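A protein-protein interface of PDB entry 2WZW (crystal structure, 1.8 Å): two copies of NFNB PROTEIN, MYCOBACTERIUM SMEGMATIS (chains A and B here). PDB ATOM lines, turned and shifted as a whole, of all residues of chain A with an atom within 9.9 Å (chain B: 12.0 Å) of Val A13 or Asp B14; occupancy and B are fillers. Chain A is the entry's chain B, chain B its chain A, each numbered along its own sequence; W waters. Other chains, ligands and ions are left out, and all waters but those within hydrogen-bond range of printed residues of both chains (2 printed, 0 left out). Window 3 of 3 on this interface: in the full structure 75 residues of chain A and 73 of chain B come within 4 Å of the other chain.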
ATOM      1  N   VAL A  13       4.797 -10.759  -4.042  1.00  0.00           N
ATOM      2  CA  VAL A  13       5.717 -10.951  -2.918  1.00  0.00           C
ATOM      3  C   VAL A  13       5.520 -12.335  -2.261  1.00  0.00           C
ATOM      4  O   VAL A  13       4.497 -12.578  -1.614  1.00  0.00           O
ATOM      5  CB  VAL A  13       5.674  -9.782  -1.883  1.00  0.00           C
ATOM      6  CG1 VAL A  13       6.761  -9.944  -0.825  1.00  0.00           C
ATOM      7  CG2 VAL A  13       5.809  -8.421  -2.568  1.00  0.00           C
ATOM      8  N   ASP A  14       6.511 -13.231  -2.450  1.00  0.00           N
ATOM      9  CA  ASP A  14       6.579 -14.591  -1.892  1.00  0.00           C
ATOM     10  C   ASP A  14       6.777 -14.479  -0.364  1.00  0.00           C
ATOM     11  O   ASP A  14       7.523 -13.597   0.067  1.00  0.00           O
ATOM     12  CB  ASP A  14       7.748 -15.337  -2.563  1.00  0.00           C
ATOM     13  CG  ASP A  14       8.196 -16.603  -1.868  1.00  0.00           C
ATOM     14  OD1 ASP A  14       7.535 -17.646  -2.059  1.00  0.00           O
ATOM     15  OD2 ASP A  14       9.220 -16.555  -1.148  1.00  0.00           O
ATOM     16  N   LEU A  15       6.087 -15.336   0.447  1.00  0.00           N
ATOM     17  CA  LEU A  15       6.136 -15.277   1.923  1.00  0.00           C
ATOM     18  C   LEU A  15       7.514 -15.414   2.548  1.00  0.00           C
ATOM     19  O   LEU A  15       7.859 -14.622   3.425  1.00  0.00           O
ATOM     20  CB  LEU A  15       5.122 -16.202   2.621  1.00  0.00           C
ATOM     21  CG  LEU A  15       3.651 -15.734   2.767  1.00  0.00           C
ATOM     22  CD1 LEU A  15       2.924 -16.575   3.805  1.00  0.00           C
ATOM     23  CD2 LEU A  15       3.534 -14.252   3.157  1.00  0.00           C
ATOM     24  N   ALA A  16       8.297 -16.402   2.102  1.00  0.00           N
ATOM     25  CA  ALA A  16       9.656 -16.628   2.598  1.00  0.00           C
ATOM     26  C   ALA A  16      10.521 -15.377   2.336  1.00  0.00           C
ATOM     27  O   ALA A  16      11.241 -14.946   3.237  1.00  0.00           O
ATOM     28  CB  ALA A  16      10.263 -17.857   1.927  1.00  0.00           C
ATOM     29  N   GLN A  17      10.413 -14.782   1.118  1.00  0.00           N
ATOM     30  CA  GLN A  17      11.161 -13.580   0.746  1.00  0.00           C
ATOM     31  C   GLN A  17      10.713 -12.385   1.597  1.00  0.00           C
ATOM     32  O   GLN A  17      11.546 -11.598   2.050  1.00  0.00           O
ATOM     33  CB  GLN A  17      10.993 -13.293  -0.754  1.00  0.00           C
ATOM     34  CG  GLN A  17      11.741 -14.293  -1.642  1.00  0.00           C
ATOM     35  CD  GLN A  17      11.332 -14.277  -3.101  1.00  0.00           C
ATOM     36  OE1 GLN A  17      10.458 -13.517  -3.542  1.00  0.00           O
ATOM     37  NE2 GLN A  17      11.963 -15.133  -3.887  1.00  0.00           N
ATOM     38  N   ALA A  18       9.397 -12.269   1.825  1.00  0.00           N
ATOM     39  CA  ALA A  18       8.818 -11.192   2.629  1.00  0.00           C
ATOM     40  C   ALA A  18       9.321 -11.233   4.081  1.00  0.00           C
ATOM     41  O   ALA A  18       9.693 -10.184   4.609  1.00  0.00           O
ATOM     42  CB  ALA A  18       7.304 -11.267   2.594  1.00  0.00           C
ATOM     43  N   ALA A  19       9.375 -12.429   4.712  1.00  0.00           N
ATOM     44  CA  ALA A  19       9.864 -12.533   6.096  1.00  0.00           C
ATOM     45  C   ALA A  19      11.343 -12.163   6.172  1.00  0.00           C
ATOM     46  O   ALA A  19      11.743 -11.501   7.121  1.00  0.00           O
ATOM     47  CB  ALA A  19       9.646 -13.938   6.652  1.00  0.00           C
ATOM     48  N   GLU A  20      12.141 -12.545   5.159  1.00  0.00           N
ATOM     49  CA  GLU A  20      13.554 -12.172   5.128  1.00  0.00           C
ATOM     50  C   GLU A  20      13.679 -10.638   5.061  1.00  0.00           C
ATOM     51  O   GLU A  20      14.428 -10.054   5.841  1.00  0.00           O
ATOM     52  CB  GLU A  20      14.257 -12.828   3.930  1.00  0.00           C
ATOM     53  CG  GLU A  20      15.701 -13.182   4.217  1.00  0.00           C
ATOM     54  CD  GLU A  20      16.439 -13.758   3.028  1.00  0.00           C
ATOM     55  OE1 GLU A  20      16.137 -14.911   2.641  1.00  0.00           O
ATOM     56  OE2 GLU A  20      17.319 -13.055   2.479  1.00  0.00           O
ATOM     57  N   ARG A  21      12.900  -9.992   4.176  1.00  0.00           N
ATOM     58  CA  ARG A  21      12.897  -8.539   4.012  1.00  0.00           C
ATOM     59  C   ARG A  21      12.486  -7.801   5.280  1.00  0.00           C
ATOM     60  O   ARG A  21      13.155  -6.849   5.662  1.00  0.00           O
ATOM     61  CB  ARG A  21      12.007  -8.124   2.839  1.00  0.00           C
ATOM     62  CG  ARG A  21      12.744  -8.271   1.513  1.00  0.00           C
ATOM     63  CD  ARG A  21      11.837  -8.000   0.339  1.00  0.00           C
ATOM     64  NE  ARG A  21      11.396  -6.606   0.244  1.00  0.00           N
ATOM     65  CZ  ARG A  21      10.362  -6.219  -0.497  1.00  0.00           C
ATOM     66  NH1 ARG A  21       9.658  -7.115  -1.188  1.00  0.00           N
ATOM     67  NH2 ARG A  21      10.013  -4.941  -0.546  1.00  0.00           N
ATOM     68  N   LEU A  22      11.415  -8.258   5.954  1.00  0.00           N
ATOM     69  CA  LEU A  22      10.973  -7.632   7.196  1.00  0.00           C
ATOM     70  C   LEU A  22      11.973  -7.824   8.334  1.00  0.00           C
ATOM     71  O   LEU A  22      12.309  -6.861   9.025  1.00  0.00           O
ATOM     72  CB  LEU A  22       9.593  -8.185   7.628  1.00  0.00           C
ATOM     73  CG  LEU A  22       8.428  -7.916   6.669  1.00  0.00           C
ATOM     74  CD1 LEU A  22       7.190  -8.668   7.085  1.00  0.00           C
ATOM     75  CD2 LEU A  22       8.162  -6.431   6.519  1.00  0.00           C
ATOM     76  N   THR A 172       7.850  -1.952   9.937  1.00  0.00           N
ATOM     77  CA  THR A 172       8.811  -2.126   8.815  1.00  0.00           C
ATOM     78  C   THR A 172       8.079  -2.409   7.489  1.00  0.00           C
ATOM     79  O   THR A 172       8.491  -1.906   6.436  1.00  0.00           O
ATOM     80  CB  THR A 172       9.827  -3.226   9.173  1.00  0.00           C
ATOM     81  OG1 THR A 172      10.537  -2.835  10.357  1.00  0.00           O
ATOM     82  CG2 THR A 172      10.836  -3.503   8.051  1.00  0.00           C
ATOM     83  N   ALA A 173       6.980  -3.191   7.561  1.00  0.00           N
ATOM     84  CA  ALA A 173       6.143  -3.526   6.400  1.00  0.00           C
ATOM     85  C   ALA A 173       5.502  -2.306   5.734  1.00  0.00           C
ATOM     86  O   ALA A 173       5.224  -2.352   4.526  1.00  0.00           O
ATOM     87  CB  ALA A 173       5.072  -4.526   6.792  1.00  0.00           C
ATOM     88  N   HIS A 174       5.281  -1.222   6.510  1.00  0.00           N
ATOM     89  CA  HIS A 174       4.706   0.032   6.014  1.00  0.00           C
ATOM     90  C   HIS A 174       5.767   1.139   5.804  1.00  0.00           C
ATOM     91  O   HIS A 174       5.416   2.311   5.610  1.00  0.00           O
ATOM     92  CB  HIS A 174       3.539   0.500   6.920  1.00  0.00           C
ATOM     93  CG  HIS A 174       2.361  -0.423   6.882  1.00  0.00           C
ATOM     94  ND1 HIS A 174       1.258  -0.157   6.077  1.00  0.00           N
ATOM     95  CD2 HIS A 174       2.176  -1.613   7.499  1.00  0.00           C
ATOM     96  CE1 HIS A 174       0.422  -1.168   6.268  1.00  0.00           C
ATOM     97  NE2 HIS A 174       0.941  -2.082   7.097  1.00  0.00           N
ATOM     98  N   ASP B  14       1.911  -7.150  -1.992  1.00  0.00           N
ATOM     99  CA  ASP B  14       2.914  -6.229  -1.466  1.00  0.00           C
ATOM    100  C   ASP B  14       3.379  -6.613  -0.048  1.00  0.00           C
ATOM    101  O   ASP B  14       2.834  -7.545   0.563  1.00  0.00           O
ATOM    102  CB  ASP B  14       2.410  -4.768  -1.535  1.00  0.00           C
ATOM    103  CG  ASP B  14       1.124  -4.468  -0.783  1.00  0.00           C
ATOM    104  OD1 ASP B  14       0.320  -3.649  -1.285  1.00  0.00           O
ATOM    105  OD2 ASP B  14       0.930  -5.031   0.324  1.00  0.00           O
ATOM    106  N   LEU B  15       4.384  -5.893   0.477  1.00  0.00           N
ATOM    107  CA  LEU B  15       4.943  -6.153   1.800  1.00  0.00           C
ATOM    108  C   LEU B  15       3.932  -6.002   2.954  1.00  0.00           C
ATOM    109  O   LEU B  15       3.972  -6.785   3.909  1.00  0.00           O
ATOM    110  CB  LEU B  15       6.178  -5.265   2.012  1.00  0.00           C
ATOM    111  CG  LEU B  15       7.287  -5.795   2.910  1.00  0.00           C
ATOM    112  CD1 LEU B  15       7.800  -7.178   2.457  1.00  0.00           C
ATOM    113  CD2 LEU B  15       8.439  -4.792   2.978  1.00  0.00           C
ATOM    114  N   ALA B  16       3.023  -5.025   2.852  1.00  0.00           N
ATOM    115  CA  ALA B  16       1.978  -4.792   3.862  1.00  0.00           C
ATOM    116  C   ALA B  16       1.069  -6.026   3.987  1.00  0.00           C
ATOM    117  O   ALA B  16       0.823  -6.492   5.104  1.00  0.00           O
ATOM    118  CB  ALA B  16       1.154  -3.566   3.491  1.00  0.00           C
ATOM    119  N   GLN B  17       0.630  -6.585   2.834  1.00  0.00           N
ATOM    120  CA  GLN B  17      -0.213  -7.789   2.775  1.00  0.00           C
ATOM    121  C   GLN B  17       0.529  -9.026   3.279  1.00  0.00           C
ATOM    122  O   GLN B  17      -0.056  -9.838   4.002  1.00  0.00           O
ATOM    123  CB  GLN B  17      -0.743  -8.014   1.353  1.00  0.00           C
ATOM    124  CG  GLN B  17      -1.962  -8.937   1.295  1.00  0.00           C
ATOM    125  CD  GLN B  17      -2.456  -9.125  -0.116  1.00  0.00           C
ATOM    126  OE1 GLN B  17      -2.132 -10.112  -0.783  1.00  0.00           O
ATOM    127  NE2 GLN B  17      -3.256  -8.183  -0.603  1.00  0.00           N
ATOM    128  N   ALA B  18       1.817  -9.180   2.888  1.00  0.00           N
ATOM    129  CA  ALA B  18       2.623 -10.300   3.338  1.00  0.00           C
ATOM    130  C   ALA B  18       2.780 -10.287   4.872  1.00  0.00           C
ATOM    131  O   ALA B  18       2.639 -11.343   5.475  1.00  0.00           O
ATOM    132  CB  ALA B  18       3.976 -10.294   2.648  1.00  0.00           C
ATOM    133  N   ALA B  19       2.995  -9.094   5.506  1.00  0.00           N
ATOM    134  CA  ALA B  19       3.098  -8.967   6.966  1.00  0.00           C
ATOM    135  C   ALA B  19       1.779  -9.379   7.635  1.00  0.00           C
ATOM    136  O   ALA B  19       1.816 -10.072   8.650  1.00  0.00           O
ATOM    137  CB  ALA B  19       3.469  -7.538   7.364  1.00  0.00           C
ATOM    138  N   GLU B  20       0.624  -8.961   7.056  1.00  0.00           N
ATOM    139  CA  GLU B  20      -0.692  -9.328   7.570  1.00  0.00           C
ATOM    140  C   GLU B  20      -0.838 -10.853   7.530  1.00  0.00           C
ATOM    141  O   GLU B  20      -1.243 -11.450   8.525  1.00  0.00           O
ATOM    142  CB  GLU B  20      -1.787  -8.666   6.725  1.00  0.00           C
ATOM    143  CG  GLU B  20      -3.145  -8.630   7.401  1.00  0.00           C
ATOM    144  CD  GLU B  20      -4.228  -7.993   6.553  1.00  0.00           C
ATOM    145  OE1 GLU B  20      -4.013  -6.859   6.066  1.00  0.00           O
ATOM    146  OE2 GLU B  20      -5.292  -8.628   6.376  1.00  0.00           O
ATOM    147  N   ARG B  21      -0.475 -11.484   6.371  1.00  0.00           N
ATOM    148  CA  ARG B  21      -0.560 -12.935   6.197  1.00  0.00           C
ATOM    149  C   ARG B  21       0.309 -13.695   7.192  1.00  0.00           C
ATOM    150  O   ARG B  21      -0.125 -14.733   7.685  1.00  0.00           O
ATOM    151  CB  ARG B  21      -0.260 -13.345   4.748  1.00  0.00           C
ATOM    152  CG  ARG B  21      -1.455 -13.123   3.829  1.00  0.00           C
ATOM    153  CD  ARG B  21      -1.061 -12.939   2.376  1.00  0.00           C
ATOM    154  NE  ARG B  21      -2.232 -12.653   1.546  1.00  0.00           N
ATOM    155  CZ  ARG B  21      -2.734 -13.479   0.633  1.00  0.00           C
ATOM    156  NH1 ARG B  21      -2.154 -14.648   0.395  1.00  0.00           N
ATOM    157  NH2 ARG B  21      -3.809 -13.134  -0.062  1.00  0.00           N
ATOM    158  N   LEU B  22       1.522 -13.184   7.502  1.00  0.00           N
ATOM    159  CA  LEU B  22       2.421 -13.845   8.458  1.00  0.00           C
ATOM    160  C   LEU B  22       1.923 -13.726   9.890  1.00  0.00           C
ATOM    161  O   LEU B  22       1.854 -14.725  10.599  1.00  0.00           O
ATOM    162  CB  LEU B  22       3.872 -13.291   8.392  1.00  0.00           C
ATOM    163  CG  LEU B  22       4.644 -13.503   7.101  1.00  0.00           C
ATOM    164  CD1 LEU B  22       5.960 -12.737   7.129  1.00  0.00           C
ATOM    165  CD2 LEU B  22       4.881 -14.978   6.850  1.00  0.00           C
ATOM    166  N   ILE B  23       1.651 -12.492  10.332  1.00  0.00           N
ATOM    167  CA  ILE B  23       1.272 -12.199  11.718  1.00  0.00           C
ATOM    168  C   ILE B  23      -0.100 -12.789  12.070  1.00  0.00           C
ATOM    169  O   ILE B  23      -0.276 -13.349  13.155  1.00  0.00           O
ATOM    170  CB  ILE B  23       1.408 -10.674  11.997  1.00  0.00           C
ATOM    171  CG1 ILE B  23       2.900 -10.255  11.890  1.00  0.00           C
ATOM    172  CG2 ILE B  23       0.816 -10.303  13.370  1.00  0.00           C
ATOM    173  CD1 ILE B  23       3.164  -8.707  11.737  1.00  0.00           C
ATOM    174  N   THR B 172       6.368 -19.611  10.034  1.00  0.00           N
ATOM    175  CA  THR B 172       5.130 -19.401   9.273  1.00  0.00           C
ATOM    176  C   THR B 172       5.426 -19.079   7.817  1.00  0.00           C
ATOM    177  O   THR B 172       4.740 -19.598   6.938  1.00  0.00           O
ATOM    178  CB  THR B 172       4.256 -18.308   9.933  1.00  0.00           C
ATOM    179  OG1 THR B 172       3.990 -18.708  11.280  1.00  0.00           O
ATOM    180  CG2 THR B 172       2.906 -18.098   9.187  1.00  0.00           C
ATOM    181  N   ALA B 173       6.475 -18.258   7.560  1.00  0.00           N
ATOM    182  CA  ALA B 173       6.862 -17.873   6.201  1.00  0.00           C
ATOM    183  C   ALA B 173       7.230 -19.063   5.319  1.00  0.00           C
ATOM    184  O   ALA B 173       7.120 -18.955   4.105  1.00  0.00           O
ATOM    185  CB  ALA B 173       8.016 -16.888   6.243  1.00  0.00           C
ATOM    186  N   HIS B 174       7.687 -20.184   5.929  1.00  0.00           N
ATOM    187  CA  HIS B 174       8.068 -21.403   5.205  1.00  0.00           C
ATOM    188  C   HIS B 174       6.990 -22.499   5.321  1.00  0.00           C
ATOM    189  O   HIS B 174       7.272 -23.672   5.062  1.00  0.00           O
ATOM    190  CB  HIS B 174       9.436 -21.902   5.715  1.00  0.00           C
ATOM    191  CG  HIS B 174      10.571 -21.023   5.278  1.00  0.00           C
ATOM    192  ND1 HIS B 174      11.268 -21.282   4.114  1.00  0.00           N
ATOM    193  CD2 HIS B 174      11.014 -19.856   5.803  1.00  0.00           C
ATOM    194  CE1 HIS B 174      12.164 -20.310   4.004  1.00  0.00           C
ATOM    195  NE2 HIS B 174      12.044 -19.421   4.989  1.00  0.00           N
HETATM  196  O   HOH W   1       0.031  -4.730   7.157  1.00  0.00           O
HETATM  197  O   HOH W   2      12.767 -16.569   4.924  1.00  0.00           O
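The side-chain carboxylate (OD2) of Asp B14 sits at hydrogen-bond distance from the backbone NH (N) of Ala B16, at 3.3 Å.
The side-chain carboxylate (OD2) of Asp A14 is in hydrogen-bond range of the backbone NH (N) of Ala A16 (3.4 Å).
The side-chain carboxylate of Asp B14 lies within hydrogen-bond range of the backbone NH of Gln B17 (3.0 Å).
The backbone carbonyl oxygen of Ala B173 is in hydrogen-bond range of the backbone NH of Ala A16 (3.5 Å).
Of the 13 printed residues of chain A, 9 touch a printed residue of chain B.
Along chain A the printed residues that touch a printed residue of chain B span positions 13 to 174.
Among the printed residues, no Asp or Glu carboxylate lies within 4 Å of a Lys or Arg side-chain nitrogen of the other chain.
Leu A15 touches Ala B18, but with the chains exchanged Ala A18 does not touch Leu B15 (4.1 Å).
Leu A15 touches Ala B173, and with the chains exchanged Ala A173 touches Leu B15.
Ala A18 touches its own counterpart, Ala B18.
Ala A19 touches Leu B22, and with the chains exchanged Leu A22 touches Ala B19.
Water W2 lies within hydrogen-bond range of the backbone carbonyl oxygen of Ala A16 and a ring nitrogen (NE2) of His B174.
Water W1 lies within hydrogen-bond range of a ring nitrogen (NE2) of His A174 and the backbone carbonyl oxygen (O) of Ala B16.
Of chain B, only Asp B14 comes within 4 Å of Val A13.
Asp B14 touches just one residue of chain A: Val A13 (3.8 Å).
No residue of chain B comes within 4 Å of Asp A14.
Leu A15 touches three residues of chain B.
Ala A18 touches just one residue of chain B: Ala B18.
Ala B16 touches just these residues of chain A: Ala A173 and His A174.
Gln B17 touches none of the printed residues of chain A.
Of the printed residues of chain A, Ala B19 touches Leu A22 (3.9 Å) and Ala A173 (3.5 Å).
Of the printed residues of chain B, Arg A21 touches Leu B15.
Of the printed residues of chain B, Leu A22 touches Leu B15 and Ala B19.
Printed residues of chain A within 4 Å of Leu B15: Arg A21 (3.9 Å), Leu A22 (3.8 Å) and Ala A173 (3.8 Å).
Of the printed residues of chain A, Ala B18 touches Leu A15 (3.8 Å) and Ala A18 (3.5 Å).
Glu B20 touches none of the printed residues of chain A.
The nearest residue of chain B that does not touch Val A13 is Leu B15 (4.2 Å).
The nearest residue of chain A that does not touch Asp B14 is Ala A18 (6.2 Å).
The nearest printed residue of chain B that does not touch Ala A16 is Leu B22 (6.0 Å).
Val A13 touches Asp B14.
Leu A15 touches Ala B18 (CD2 to O, 3.8 Å).
CD2 of Leu B22 touches CD1 of Leu A15, 3.96 Å away.
Leu A15 touches Ala B173 (O to CB, 3.6 Å).
CB of Ala B18 touches CB of Ala A18, at 3.5 Å.
CB of Ala A19 touches CD1 of Leu B22 (3.9 Å).
Leu A22 touches Leu B15.
CB of Ala A173 touches O of Leu B15, at 3.8 Å.
O of Ala A173 touches N of Ala B16, at 3.8 Å.
CB of Ala A173 touches CB of Ala B19 (3.5 Å).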
